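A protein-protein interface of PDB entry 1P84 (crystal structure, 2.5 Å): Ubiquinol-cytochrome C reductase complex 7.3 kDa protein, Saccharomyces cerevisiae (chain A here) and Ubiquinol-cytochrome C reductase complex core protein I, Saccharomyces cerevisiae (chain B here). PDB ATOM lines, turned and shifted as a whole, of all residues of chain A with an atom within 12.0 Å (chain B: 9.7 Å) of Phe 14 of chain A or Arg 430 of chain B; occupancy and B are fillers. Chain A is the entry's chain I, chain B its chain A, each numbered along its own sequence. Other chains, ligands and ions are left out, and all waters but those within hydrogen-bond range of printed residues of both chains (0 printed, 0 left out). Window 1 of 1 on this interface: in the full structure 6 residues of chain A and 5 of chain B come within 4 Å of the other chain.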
ATOM      1  N   TYR A   4       3.490 -27.376 -19.389  1.00  0.00           N
ATOM      2  CA  TYR A   4       2.883 -26.167 -19.924  1.00  0.00           C
ATOM      3  C   TYR A   4       3.515 -24.925 -19.287  1.00  0.00           C
ATOM      4  O   TYR A   4       3.917 -23.996 -19.989  1.00  0.00           O
ATOM      5  CB  TYR A   4       1.361 -26.179 -19.685  1.00  0.00           C
ATOM      6  CG  TYR A   4       0.635 -24.971 -20.248  1.00  0.00           C
ATOM      7  CD1 TYR A   4       0.377 -23.852 -19.451  1.00  0.00           C
ATOM      8  CD2 TYR A   4       0.252 -24.926 -21.592  1.00  0.00           C
ATOM      9  CE1 TYR A   4      -0.232 -22.718 -19.977  1.00  0.00           C
ATOM     10  CE2 TYR A   4      -0.360 -23.795 -22.126  1.00  0.00           C
ATOM     11  CZ  TYR A   4      -0.595 -22.697 -21.315  1.00  0.00           C
ATOM     12  OH  TYR A   4      -1.176 -21.569 -21.839  1.00  0.00           O
ATOM     13  N   LYS A   5       3.631 -24.937 -17.961  1.00  0.00           N
ATOM     14  CA  LYS A   5       4.194 -23.815 -17.210  1.00  0.00           C
ATOM     15  C   LYS A   5       5.643 -23.454 -17.549  1.00  0.00           C
ATOM     16  O   LYS A   5       6.135 -22.404 -17.131  1.00  0.00           O
ATOM     17  CB  LYS A   5       4.050 -24.060 -15.704  1.00  0.00           C
ATOM     18  CG  LYS A   5       2.609 -24.092 -15.215  1.00  0.00           C
ATOM     19  CD  LYS A   5       2.514 -24.398 -13.724  1.00  0.00           C
ATOM     20  CE  LYS A   5       3.135 -23.296 -12.874  1.00  0.00           C
ATOM     21  NZ  LYS A   5       2.991 -23.578 -11.415  1.00  0.00           N
ATOM     22  N   THR A   6       6.329 -24.315 -18.294  1.00  0.00           N
ATOM     23  CA  THR A   6       7.713 -24.042 -18.673  1.00  0.00           C
ATOM     24  C   THR A   6       7.797 -23.148 -19.912  1.00  0.00           C
ATOM     25  O   THR A   6       8.701 -22.316 -20.019  1.00  0.00           O
ATOM     26  CB  THR A   6       8.518 -25.344 -18.916  1.00  0.00           C
ATOM     27  OG1 THR A   6       7.840 -26.161 -19.877  1.00  0.00           O
ATOM     28  CG2 THR A   6       8.681 -26.124 -17.620  1.00  0.00           C
ATOM     29  N   PHE A   7       6.840 -23.310 -20.827  1.00  0.00           N
ATOM     30  CA  PHE A   7       6.799 -22.526 -22.061  1.00  0.00           C
ATOM     31  C   PHE A   7       5.945 -21.263 -21.975  1.00  0.00           C
ATOM     32  O   PHE A   7       6.338 -20.207 -22.477  1.00  0.00           O
ATOM     33  CB  PHE A   7       6.253 -23.357 -23.220  1.00  0.00           C
ATOM     34  CG  PHE A   7       7.048 -24.588 -23.528  1.00  0.00           C
ATOM     35  CD1 PHE A   7       8.148 -24.528 -24.379  1.00  0.00           C
ATOM     36  CD2 PHE A   7       6.659 -25.825 -23.019  1.00  0.00           C
ATOM     37  CE1 PHE A   7       8.848 -25.684 -24.722  1.00  0.00           C
ATOM     38  CE2 PHE A   7       7.348 -26.986 -23.353  1.00  0.00           C
ATOM     39  CZ  PHE A   7       8.444 -26.918 -24.208  1.00  0.00           C
ATOM     40  N   PHE A   8       4.775 -21.377 -21.351  1.00  0.00           N
ATOM     41  CA  PHE A   8       3.844 -20.254 -21.264  1.00  0.00           C
ATOM     42  C   PHE A   8       3.625 -19.627 -19.887  1.00  0.00           C
ATOM     43  O   PHE A   8       3.089 -18.520 -19.792  1.00  0.00           O
ATOM     44  CB  PHE A   8       2.518 -20.661 -21.918  1.00  0.00           C
ATOM     45  CG  PHE A   8       2.695 -21.330 -23.261  1.00  0.00           C
ATOM     46  CD1 PHE A   8       2.991 -20.579 -24.397  1.00  0.00           C
ATOM     47  CD2 PHE A   8       2.627 -22.716 -23.376  1.00  0.00           C
ATOM     48  CE1 PHE A   8       3.225 -21.203 -25.626  1.00  0.00           C
ATOM     49  CE2 PHE A   8       2.859 -23.350 -24.604  1.00  0.00           C
ATOM     50  CZ  PHE A   8       3.158 -22.589 -25.726  1.00  0.00           C
ATOM     51  N   LYS A   9       4.020 -20.341 -18.833  1.00  0.00           N
ATOM     52  CA  LYS A   9       3.925 -19.865 -17.445  1.00  0.00           C
ATOM     53  C   LYS A   9       2.600 -19.217 -17.032  1.00  0.00           C
ATOM     54  O   LYS A   9       2.473 -17.991 -17.037  1.00  0.00           O
ATOM     55  CB  LYS A   9       5.074 -18.886 -17.149  1.00  0.00           C
ATOM     56  CG  LYS A   9       6.452 -19.392 -17.546  1.00  0.00           C
ATOM     57  CD  LYS A   9       7.482 -18.281 -17.497  1.00  0.00           C
ATOM     58  CE  LYS A   9       8.773 -18.712 -18.187  1.00  0.00           C
ATOM     59  NZ  LYS A   9       9.767 -17.599 -18.295  1.00  0.00           N
ATOM     60  N   ARG A  10       1.644 -20.045 -16.623  1.00  0.00           N
ATOM     61  CA  ARG A  10       0.311 -19.611 -16.181  1.00  0.00           C
ATOM     62  C   ARG A  10      -0.491 -18.610 -17.051  1.00  0.00           C
ATOM     63  O   ARG A  10      -1.546 -18.115 -16.635  1.00  0.00           O
ATOM     64  CB  ARG A  10       0.326 -19.171 -14.703  1.00  0.00           C
ATOM     65  CG  ARG A  10       0.708 -17.724 -14.434  1.00  0.00           C
ATOM     66  CD  ARG A  10       0.040 -17.202 -13.152  1.00  0.00           C
ATOM     67  NE  ARG A  10       0.535 -17.845 -11.934  1.00  0.00           N
ATOM     68  CZ  ARG A  10      -0.231 -18.452 -11.027  1.00  0.00           C
ATOM     69  NH1 ARG A  10       0.325 -18.997  -9.952  1.00  0.00           N
ATOM     70  NH2 ARG A  10      -1.546 -18.536 -11.193  1.00  0.00           N
ATOM     71  N   ASN A  11       0.001 -18.326 -18.254  1.00  0.00           N
ATOM     72  CA  ASN A  11      -0.681 -17.428 -19.183  1.00  0.00           C
ATOM     73  C   ASN A  11      -1.110 -18.241 -20.395  1.00  0.00           C
ATOM     74  O   ASN A  11      -0.555 -19.308 -20.664  1.00  0.00           O
ATOM     75  CB  ASN A  11       0.247 -16.298 -19.636  1.00  0.00           C
ATOM     76  CG  ASN A  11       0.040 -15.013 -18.857  1.00  0.00           C
ATOM     77  OD1 ASN A  11       0.680 -14.007 -19.135  1.00  0.00           O
ATOM     78  ND2 ASN A  11      -0.853 -15.044 -17.874  1.00  0.00           N
ATOM     79  N   ALA A  12      -2.108 -17.746 -21.120  1.00  0.00           N
ATOM     80  CA  ALA A  12      -2.589 -18.434 -22.313  1.00  0.00           C
ATOM     81  C   ALA A  12      -1.612 -18.208 -23.465  1.00  0.00           C
ATOM     82  O   ALA A  12      -0.686 -17.402 -23.355  1.00  0.00           O
ATOM     83  CB  ALA A  12      -3.976 -17.927 -22.687  1.00  0.00           C
ATOM     84  N   VAL A  13      -1.799 -18.947 -24.554  1.00  0.00           N
ATOM     85  CA  VAL A  13      -0.949 -18.802 -25.726  1.00  0.00           C
ATOM     86  C   VAL A  13      -1.456 -17.593 -26.519  1.00  0.00           C
ATOM     87  O   VAL A  13      -2.658 -17.446 -26.722  1.00  0.00           O
ATOM     88  CB  VAL A  13      -0.982 -20.068 -26.583  1.00  0.00           C
ATOM     89  CG1 VAL A  13       0.093 -20.014 -27.645  1.00  0.00           C
ATOM     90  CG2 VAL A  13      -0.792 -21.288 -25.709  1.00  0.00           C
ATOM     91  N   PHE A  14      -0.544 -16.719 -26.943  1.00  0.00           N
ATOM     92  CA  PHE A  14      -0.905 -15.506 -27.680  1.00  0.00           C
ATOM     93  C   PHE A  14      -1.052 -15.710 -29.191  1.00  0.00           C
ATOM     94  O   PHE A  14      -0.421 -16.607 -29.763  1.00  0.00           O
ATOM     95  CB  PHE A  14       0.120 -14.405 -27.378  1.00  0.00           C
ATOM     96  CG  PHE A  14       0.359 -14.187 -25.898  1.00  0.00           C
ATOM     97  CD1 PHE A  14       1.592 -14.482 -25.328  1.00  0.00           C
ATOM     98  CD2 PHE A  14      -0.660 -13.713 -25.072  1.00  0.00           C
ATOM     99  CE1 PHE A  14       1.807 -14.314 -23.954  1.00  0.00           C
ATOM    100  CE2 PHE A  14      -0.455 -13.540 -23.696  1.00  0.00           C
ATOM    101  CZ  PHE A  14       0.781 -13.843 -23.138  1.00  0.00           C
ATOM    102  N   VAL A  15      -1.866 -14.862 -29.831  1.00  0.00           N
ATOM    103  CA  VAL A  15      -2.118 -14.943 -31.280  1.00  0.00           C
ATOM    104  C   VAL A  15      -0.876 -15.176 -32.121  1.00  0.00           C
ATOM    105  O   VAL A  15      -0.888 -16.037 -32.998  1.00  0.00           O
ATOM    106  CB  VAL A  15      -2.799 -13.677 -31.870  1.00  0.00           C
ATOM    107  CG1 VAL A  15      -4.115 -14.045 -32.541  1.00  0.00           C
ATOM    108  CG2 VAL A  15      -2.980 -12.598 -30.820  1.00  0.00           C
ATOM    109  N   GLY A  16       0.175 -14.391 -31.866  1.00  0.00           N
ATOM    110  CA  GLY A  16       1.417 -14.509 -32.613  1.00  0.00           C
ATOM    111  C   GLY A  16       2.002 -15.906 -32.606  1.00  0.00           C
ATOM    112  O   GLY A  16       2.387 -16.435 -33.654  1.00  0.00           O
ATOM    113  N   THR A  17       2.054 -16.511 -31.423  1.00  0.00           N
ATOM    114  CA  THR A  17       2.578 -17.863 -31.261  1.00  0.00           C
ATOM    115  C   THR A  17       1.630 -18.873 -31.915  1.00  0.00           C
ATOM    116  O   THR A  17       2.060 -19.945 -32.354  1.00  0.00           O
ATOM    117  CB  THR A  17       2.744 -18.212 -29.763  1.00  0.00           C
ATOM    118  OG1 THR A  17       3.589 -17.233 -29.143  1.00  0.00           O
ATOM    119  CG2 THR A  17       3.351 -19.607 -29.582  1.00  0.00           C
ATOM    120  N   ILE A  18       0.339 -18.534 -31.949  1.00  0.00           N
ATOM    121  CA  ILE A  18      -0.678 -19.389 -32.558  1.00  0.00           C
ATOM    122  C   ILE A  18      -0.483 -19.363 -34.075  1.00  0.00           C
ATOM    123  O   ILE A  18      -0.354 -20.414 -34.708  1.00  0.00           O
ATOM    124  CB  ILE A  18      -2.121 -18.904 -32.223  1.00  0.00           C
ATOM    125  CG1 ILE A  18      -2.407 -19.014 -30.722  1.00  0.00           C
ATOM    126  CG2 ILE A  18      -3.141 -19.702 -33.011  1.00  0.00           C
ATOM    127  CD1 ILE A  18      -2.378 -20.423 -30.199  1.00  0.00           C
ATOM    128  N   PHE A  19      -0.437 -18.160 -34.645  1.00  0.00           N
ATOM    129  CA  PHE A  19      -0.247 -17.998 -36.082  1.00  0.00           C
ATOM    130  C   PHE A  19       1.043 -18.665 -36.537  1.00  0.00           C
ATOM    131  O   PHE A  19       1.049 -19.394 -37.524  1.00  0.00           O
ATOM    132  CB  PHE A  19      -0.230 -16.516 -36.474  1.00  0.00           C
ATOM    133  CG  PHE A  19      -1.592 -15.866 -36.484  1.00  0.00           C
ATOM    134  CD1 PHE A  19      -2.754 -16.630 -36.395  1.00  0.00           C
ATOM    135  CD2 PHE A  19      -1.713 -14.484 -36.597  1.00  0.00           C
ATOM    136  CE1 PHE A  19      -4.018 -16.028 -36.421  1.00  0.00           C
ATOM    137  CE2 PHE A  19      -2.973 -13.871 -36.624  1.00  0.00           C
ATOM    138  CZ  PHE A  19      -4.127 -14.648 -36.536  1.00  0.00           C
ATOM    139  N   ALA A  20       2.121 -18.444 -35.791  1.00  0.00           N
ATOM    140  CA  ALA A  20       3.419 -19.031 -36.114  1.00  0.00           C
ATOM    141  C   ALA A  20       3.343 -20.554 -36.127  1.00  0.00           C
ATOM    142  O   ALA A  20       3.839 -21.203 -37.047  1.00  0.00           O
ATOM    143  CB  ALA A  20       4.469 -18.567 -35.114  1.00  0.00           C
ATOM    144  N   GLY A  21       2.711 -21.116 -35.102  1.00  0.00           N
ATOM    145  CA  GLY A  21       2.565 -22.558 -35.017  1.00  0.00           C
ATOM    146  C   GLY A  21       1.720 -23.117 -36.150  1.00  0.00           C
ATOM    147  O   GLY A  21       1.998 -24.208 -36.650  1.00  0.00           O
ATOM    148  N   ALA A  22       0.703 -22.358 -36.565  1.00  0.00           N
ATOM    149  CA  ALA A  22      -0.199 -22.759 -37.647  1.00  0.00           C
ATOM    150  C   ALA A  22       0.548 -22.942 -38.965  1.00  0.00           C
ATOM    151  O   ALA A  22       0.287 -23.895 -39.699  1.00  0.00           O
ATOM    152  CB  ALA A  22      -1.320 -21.733 -37.811  1.00  0.00           C
ATOM    153  N   PHE A  23       1.479 -22.034 -39.255  1.00  0.00           N
ATOM    154  CA  PHE A  23       2.276 -22.110 -40.481  1.00  0.00           C
ATOM    155  C   PHE A  23       3.197 -23.337 -40.473  1.00  0.00           C
ATOM    156  O   PHE A  23       3.428 -23.963 -41.512  1.00  0.00           O
ATOM    157  CB  PHE A  23       3.104 -20.833 -40.677  1.00  0.00           C
ATOM    158  CG  PHE A  23       2.298 -19.639 -41.133  1.00  0.00           C
ATOM    159  CD1 PHE A  23       2.651 -18.949 -42.295  1.00  0.00           C
ATOM    160  CD2 PHE A  23       1.205 -19.184 -40.392  1.00  0.00           C
ATOM    161  CE1 PHE A  23       1.926 -17.817 -42.713  1.00  0.00           C
ATOM    162  CE2 PHE A  23       0.474 -18.057 -40.797  1.00  0.00           C
ATOM    163  CZ  PHE A  23       0.836 -17.374 -41.959  1.00  0.00           C
ATOM    164  N   THR B 329      -0.462  -3.829 -13.611  1.00  0.00           N
ATOM    165  CA  THR B 329       0.500  -4.799 -14.116  1.00  0.00           C
ATOM    166  C   THR B 329       1.277  -4.271 -15.315  1.00  0.00           C
ATOM    167  O   THR B 329       2.446  -4.616 -15.504  1.00  0.00           O
ATOM    168  CB  THR B 329      -0.194  -6.124 -14.554  1.00  0.00           C
ATOM    169  OG1 THR B 329      -0.817  -6.739 -13.424  1.00  0.00           O
ATOM    170  CG2 THR B 329       0.805  -7.117 -15.149  1.00  0.00           C
ATOM    171  N   ILE B 330       0.651  -3.402 -16.102  1.00  0.00           N
ATOM    172  CA  ILE B 330       1.291  -2.921 -17.324  1.00  0.00           C
ATOM    173  C   ILE B 330       1.540  -1.427 -17.549  1.00  0.00           C
ATOM    174  O   ILE B 330       2.502  -1.085 -18.235  1.00  0.00           O
ATOM    175  CB  ILE B 330       0.509  -3.414 -18.572  1.00  0.00           C
ATOM    176  CG1 ILE B 330      -0.879  -2.767 -18.595  1.00  0.00           C
ATOM    177  CG2 ILE B 330       0.368  -4.928 -18.562  1.00  0.00           C
ATOM    178  CD1 ILE B 330      -1.627  -2.927 -19.902  1.00  0.00           C
ATOM    179  N   TRP B 401      -3.287 -10.112 -12.072  1.00  0.00           N
ATOM    180  CA  TRP B 401      -3.368 -10.574 -13.459  1.00  0.00           C
ATOM    181  C   TRP B 401      -3.787 -12.028 -13.681  1.00  0.00           C
ATOM    182  O   TRP B 401      -3.041 -12.960 -13.364  1.00  0.00           O
ATOM    183  CB  TRP B 401      -2.056 -10.294 -14.197  1.00  0.00           C
ATOM    184  CG  TRP B 401      -2.159 -10.389 -15.708  1.00  0.00           C
ATOM    185  CD1 TRP B 401      -1.862 -11.476 -16.490  1.00  0.00           C
ATOM    186  CD2 TRP B 401      -2.526  -9.335 -16.612  1.00  0.00           C
ATOM    187  NE1 TRP B 401      -2.013 -11.157 -17.824  1.00  0.00           N
ATOM    188  CE2 TRP B 401      -2.419  -9.851 -17.924  1.00  0.00           C
ATOM    189  CE3 TRP B 401      -2.932  -8.005 -16.440  1.00  0.00           C
ATOM    190  CZ2 TRP B 401      -2.698  -9.080 -19.056  1.00  0.00           C
ATOM    191  CZ3 TRP B 401      -3.210  -7.239 -17.566  1.00  0.00           C
ATOM    192  CH2 TRP B 401      -3.091  -7.783 -18.860  1.00  0.00           C
ATOM    193  N   ASP B 402      -4.974 -12.201 -14.267  1.00  0.00           N
ATOM    194  CA  ASP B 402      -5.530 -13.517 -14.574  1.00  0.00           C
ATOM    195  C   ASP B 402      -5.575 -14.423 -13.343  1.00  0.00           C
ATOM    196  O   ASP B 402      -5.126 -15.571 -13.377  1.00  0.00           O
ATOM    197  CB  ASP B 402      -4.719 -14.160 -15.709  1.00  0.00           C
ATOM    198  CG  ASP B 402      -5.422 -15.338 -16.358  1.00  0.00           C
ATOM    199  OD1 ASP B 402      -6.632 -15.543 -16.161  1.00  0.00           O
ATOM    200  OD2 ASP B 402      -4.749 -16.077 -17.094  1.00  0.00           O
ATOM    201  N   SER B 427      -7.792  -9.490 -16.956  1.00  0.00           N
ATOM    202  CA  SER B 427      -6.712  -9.449 -17.938  1.00  0.00           C
ATOM    203  C   SER B 427      -7.103  -8.709 -19.209  1.00  0.00           C
ATOM    204  O   SER B 427      -8.192  -8.149 -19.304  1.00  0.00           O
ATOM    205  CB  SER B 427      -6.232 -10.860 -18.277  1.00  0.00           C
ATOM    206  OG  SER B 427      -7.308 -11.682 -18.670  1.00  0.00           O
ATOM    207  N   MET B 428      -6.177  -8.665 -20.163  1.00  0.00           N
ATOM    208  CA  MET B 428      -6.397  -7.998 -21.438  1.00  0.00           C
ATOM    209  C   MET B 428      -5.799  -8.814 -22.566  1.00  0.00           C
ATOM    210  O   MET B 428      -4.862  -9.580 -22.356  1.00  0.00           O
ATOM    211  CB  MET B 428      -5.727  -6.630 -21.444  1.00  0.00           C
ATOM    212  CG  MET B 428      -6.300  -5.629 -20.475  1.00  0.00           C
ATOM    213  SD  MET B 428      -5.355  -4.106 -20.571  1.00  0.00           S
ATOM    214  CE  MET B 428      -6.334  -3.198 -21.773  1.00  0.00           C
ATOM    215  N   MET B 429      -6.356  -8.652 -23.764  1.00  0.00           N
ATOM    216  CA  MET B 429      -5.866  -9.343 -24.956  1.00  0.00           C
ATOM    217  C   MET B 429      -4.586  -8.634 -25.410  1.00  0.00           C
ATOM    218  O   MET B 429      -4.427  -7.429 -25.200  1.00  0.00           O
ATOM    219  CB  MET B 429      -6.908  -9.261 -26.085  1.00  0.00           C
ATOM    220  CG  MET B 429      -8.259  -9.912 -25.798  1.00  0.00           C
ATOM    221  SD  MET B 429      -8.212 -11.711 -25.811  1.00  0.00           S
ATOM    222  CE  MET B 429      -7.876 -12.047 -27.559  1.00  0.00           C
ATOM    223  N   ARG B 430      -3.678  -9.382 -26.027  1.00  0.00           N
ATOM    224  CA  ARG B 430      -2.422  -8.823 -26.525  1.00  0.00           C
ATOM    225  C   ARG B 430      -1.851  -9.691 -27.650  1.00  0.00           C
ATOM    226  O   ARG B 430      -2.280 -10.834 -27.833  1.00  0.00           O
ATOM    227  CB  ARG B 430      -1.411  -8.670 -25.376  1.00  0.00           C
ATOM    228  CG  ARG B 430      -1.257  -9.897 -24.490  1.00  0.00           C
ATOM    229  CD  ARG B 430      -0.315  -9.646 -23.308  1.00  0.00           C
ATOM    230  NE  ARG B 430       1.063  -9.348 -23.717  1.00  0.00           N
ATOM    231  CZ  ARG B 430       1.840 -10.151 -24.451  1.00  0.00           C
ATOM    232  NH1 ARG B 430       3.077  -9.776 -24.763  1.00  0.00           N
ATOM    233  NH2 ARG B 430       1.387 -11.321 -24.886  1.00  0.00           N
ATOM    234  N   TRP B 431      -0.932  -9.130 -28.436  1.00  0.00           N
ATOM    235  CA  TRP B 431      -0.309  -9.870 -29.539  1.00  0.00           C
ATOM    236  C   TRP B 431       0.824 -10.783 -29.038  1.00  0.00           C
ATOM    237  O   TRP B 431       0.887 -11.959 -29.481  1.00  0.00           O
ATOM    238  CB  TRP B 431       0.215  -8.908 -30.613  1.00  0.00           C
ATOM    239  CG  TRP B 431       0.634  -9.594 -31.902  1.00  0.00           C
ATOM    240  CD1 TRP B 431       1.863 -10.136 -32.193  1.00  0.00           C
ATOM    241  CD2 TRP B 431      -0.183  -9.815 -33.069  1.00  0.00           C
ATOM    242  NE1 TRP B 431       1.857 -10.680 -33.460  1.00  0.00           N
ATOM    243  CE2 TRP B 431       0.617 -10.498 -34.019  1.00  0.00           C
ATOM    244  CE3 TRP B 431      -1.513  -9.504 -33.400  1.00  0.00           C
ATOM    245  CZ2 TRP B 431       0.129 -10.877 -35.277  1.00  0.00           C
ATOM    246  CZ3 TRP B 431      -1.999  -9.883 -34.655  1.00  0.00           C
ATOM    247  CH2 TRP B 431      -1.176 -10.561 -35.576  1.00  0.00           C
ATOM    248  OXT TRP B 431       1.625 -10.314 -28.193  1.00  0.00           O
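Printed residues of chain B within 4 Å of Arg 10 of chain A: Asp 402.
No residue of chain B comes within 4 Å of Ala 12 of chain A.
No residue of chain B comes within 4 Å of Val 13 of chain A.
Phe 14 of chain A touches just these residues of chain B: Arg 430 (3.1 Å) and Trp 431 (3.3 Å).
Printed residues of chain B within 4 Å of Val 15 of chain A: Arg 430.
Gly 16 of chain A touches one residue of chain B.
Printed residues of chain A within 4 Å of Asp 402 of chain B: Arg 10 (3.8 Å).
Met 429 of chain B touches none of the printed residues of chain A.
Of chain A, only Phe 14 (3.1 Å) and Val 15 (3.5 Å) come within 4 Å of Arg 430 of chain B.
The nearest residue of chain B that does not touch Phe 14 of chain A is Met 428 of chain B (6.1 Å).
N of Gly 16 of chain A sits at hydrogen-bond distance from O of Trp 431 of chain B, 3.5 Å away.
Hydrophobic or aromatic side chains of chain B that line the printed part of chain A: Trp 401 and Trp 431.
Along chain B the printed residues that touch a printed residue of chain A span positions 401 to 431.
Printed residues of chain A that touch a printed residue of chain B: Arg 10, Asn 11, Phe 14, Val 15, Gly 16 and Phe 19.
Hydrophobic or aromatic side chains of chain A within 4 Å of the printed part of chain B: Phe 14, Val 15 and Phe 19.
Among the printed residues, 7 pairs touch across the chains.
The side-chain hydroxyl (OH) of Tyr 4 of chain A sits at hydrogen-bond distance from the backbone carbonyl oxygen (O) of Asn 11 of chain A.
Among the printed residues, pairs that only touch across the chains: Phe 14 of chain A with Arg 430 of chain B, Phe 14 of chain A with Trp 431 of chain B, Val 15 of chain A with Arg 430 of chain B, Arg 10 of chain A with Asp 402 of chain B, Phe 19 of chain A with Trp 431 of chain B and Asn 11 of chain A with Trp 401 of chain B.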
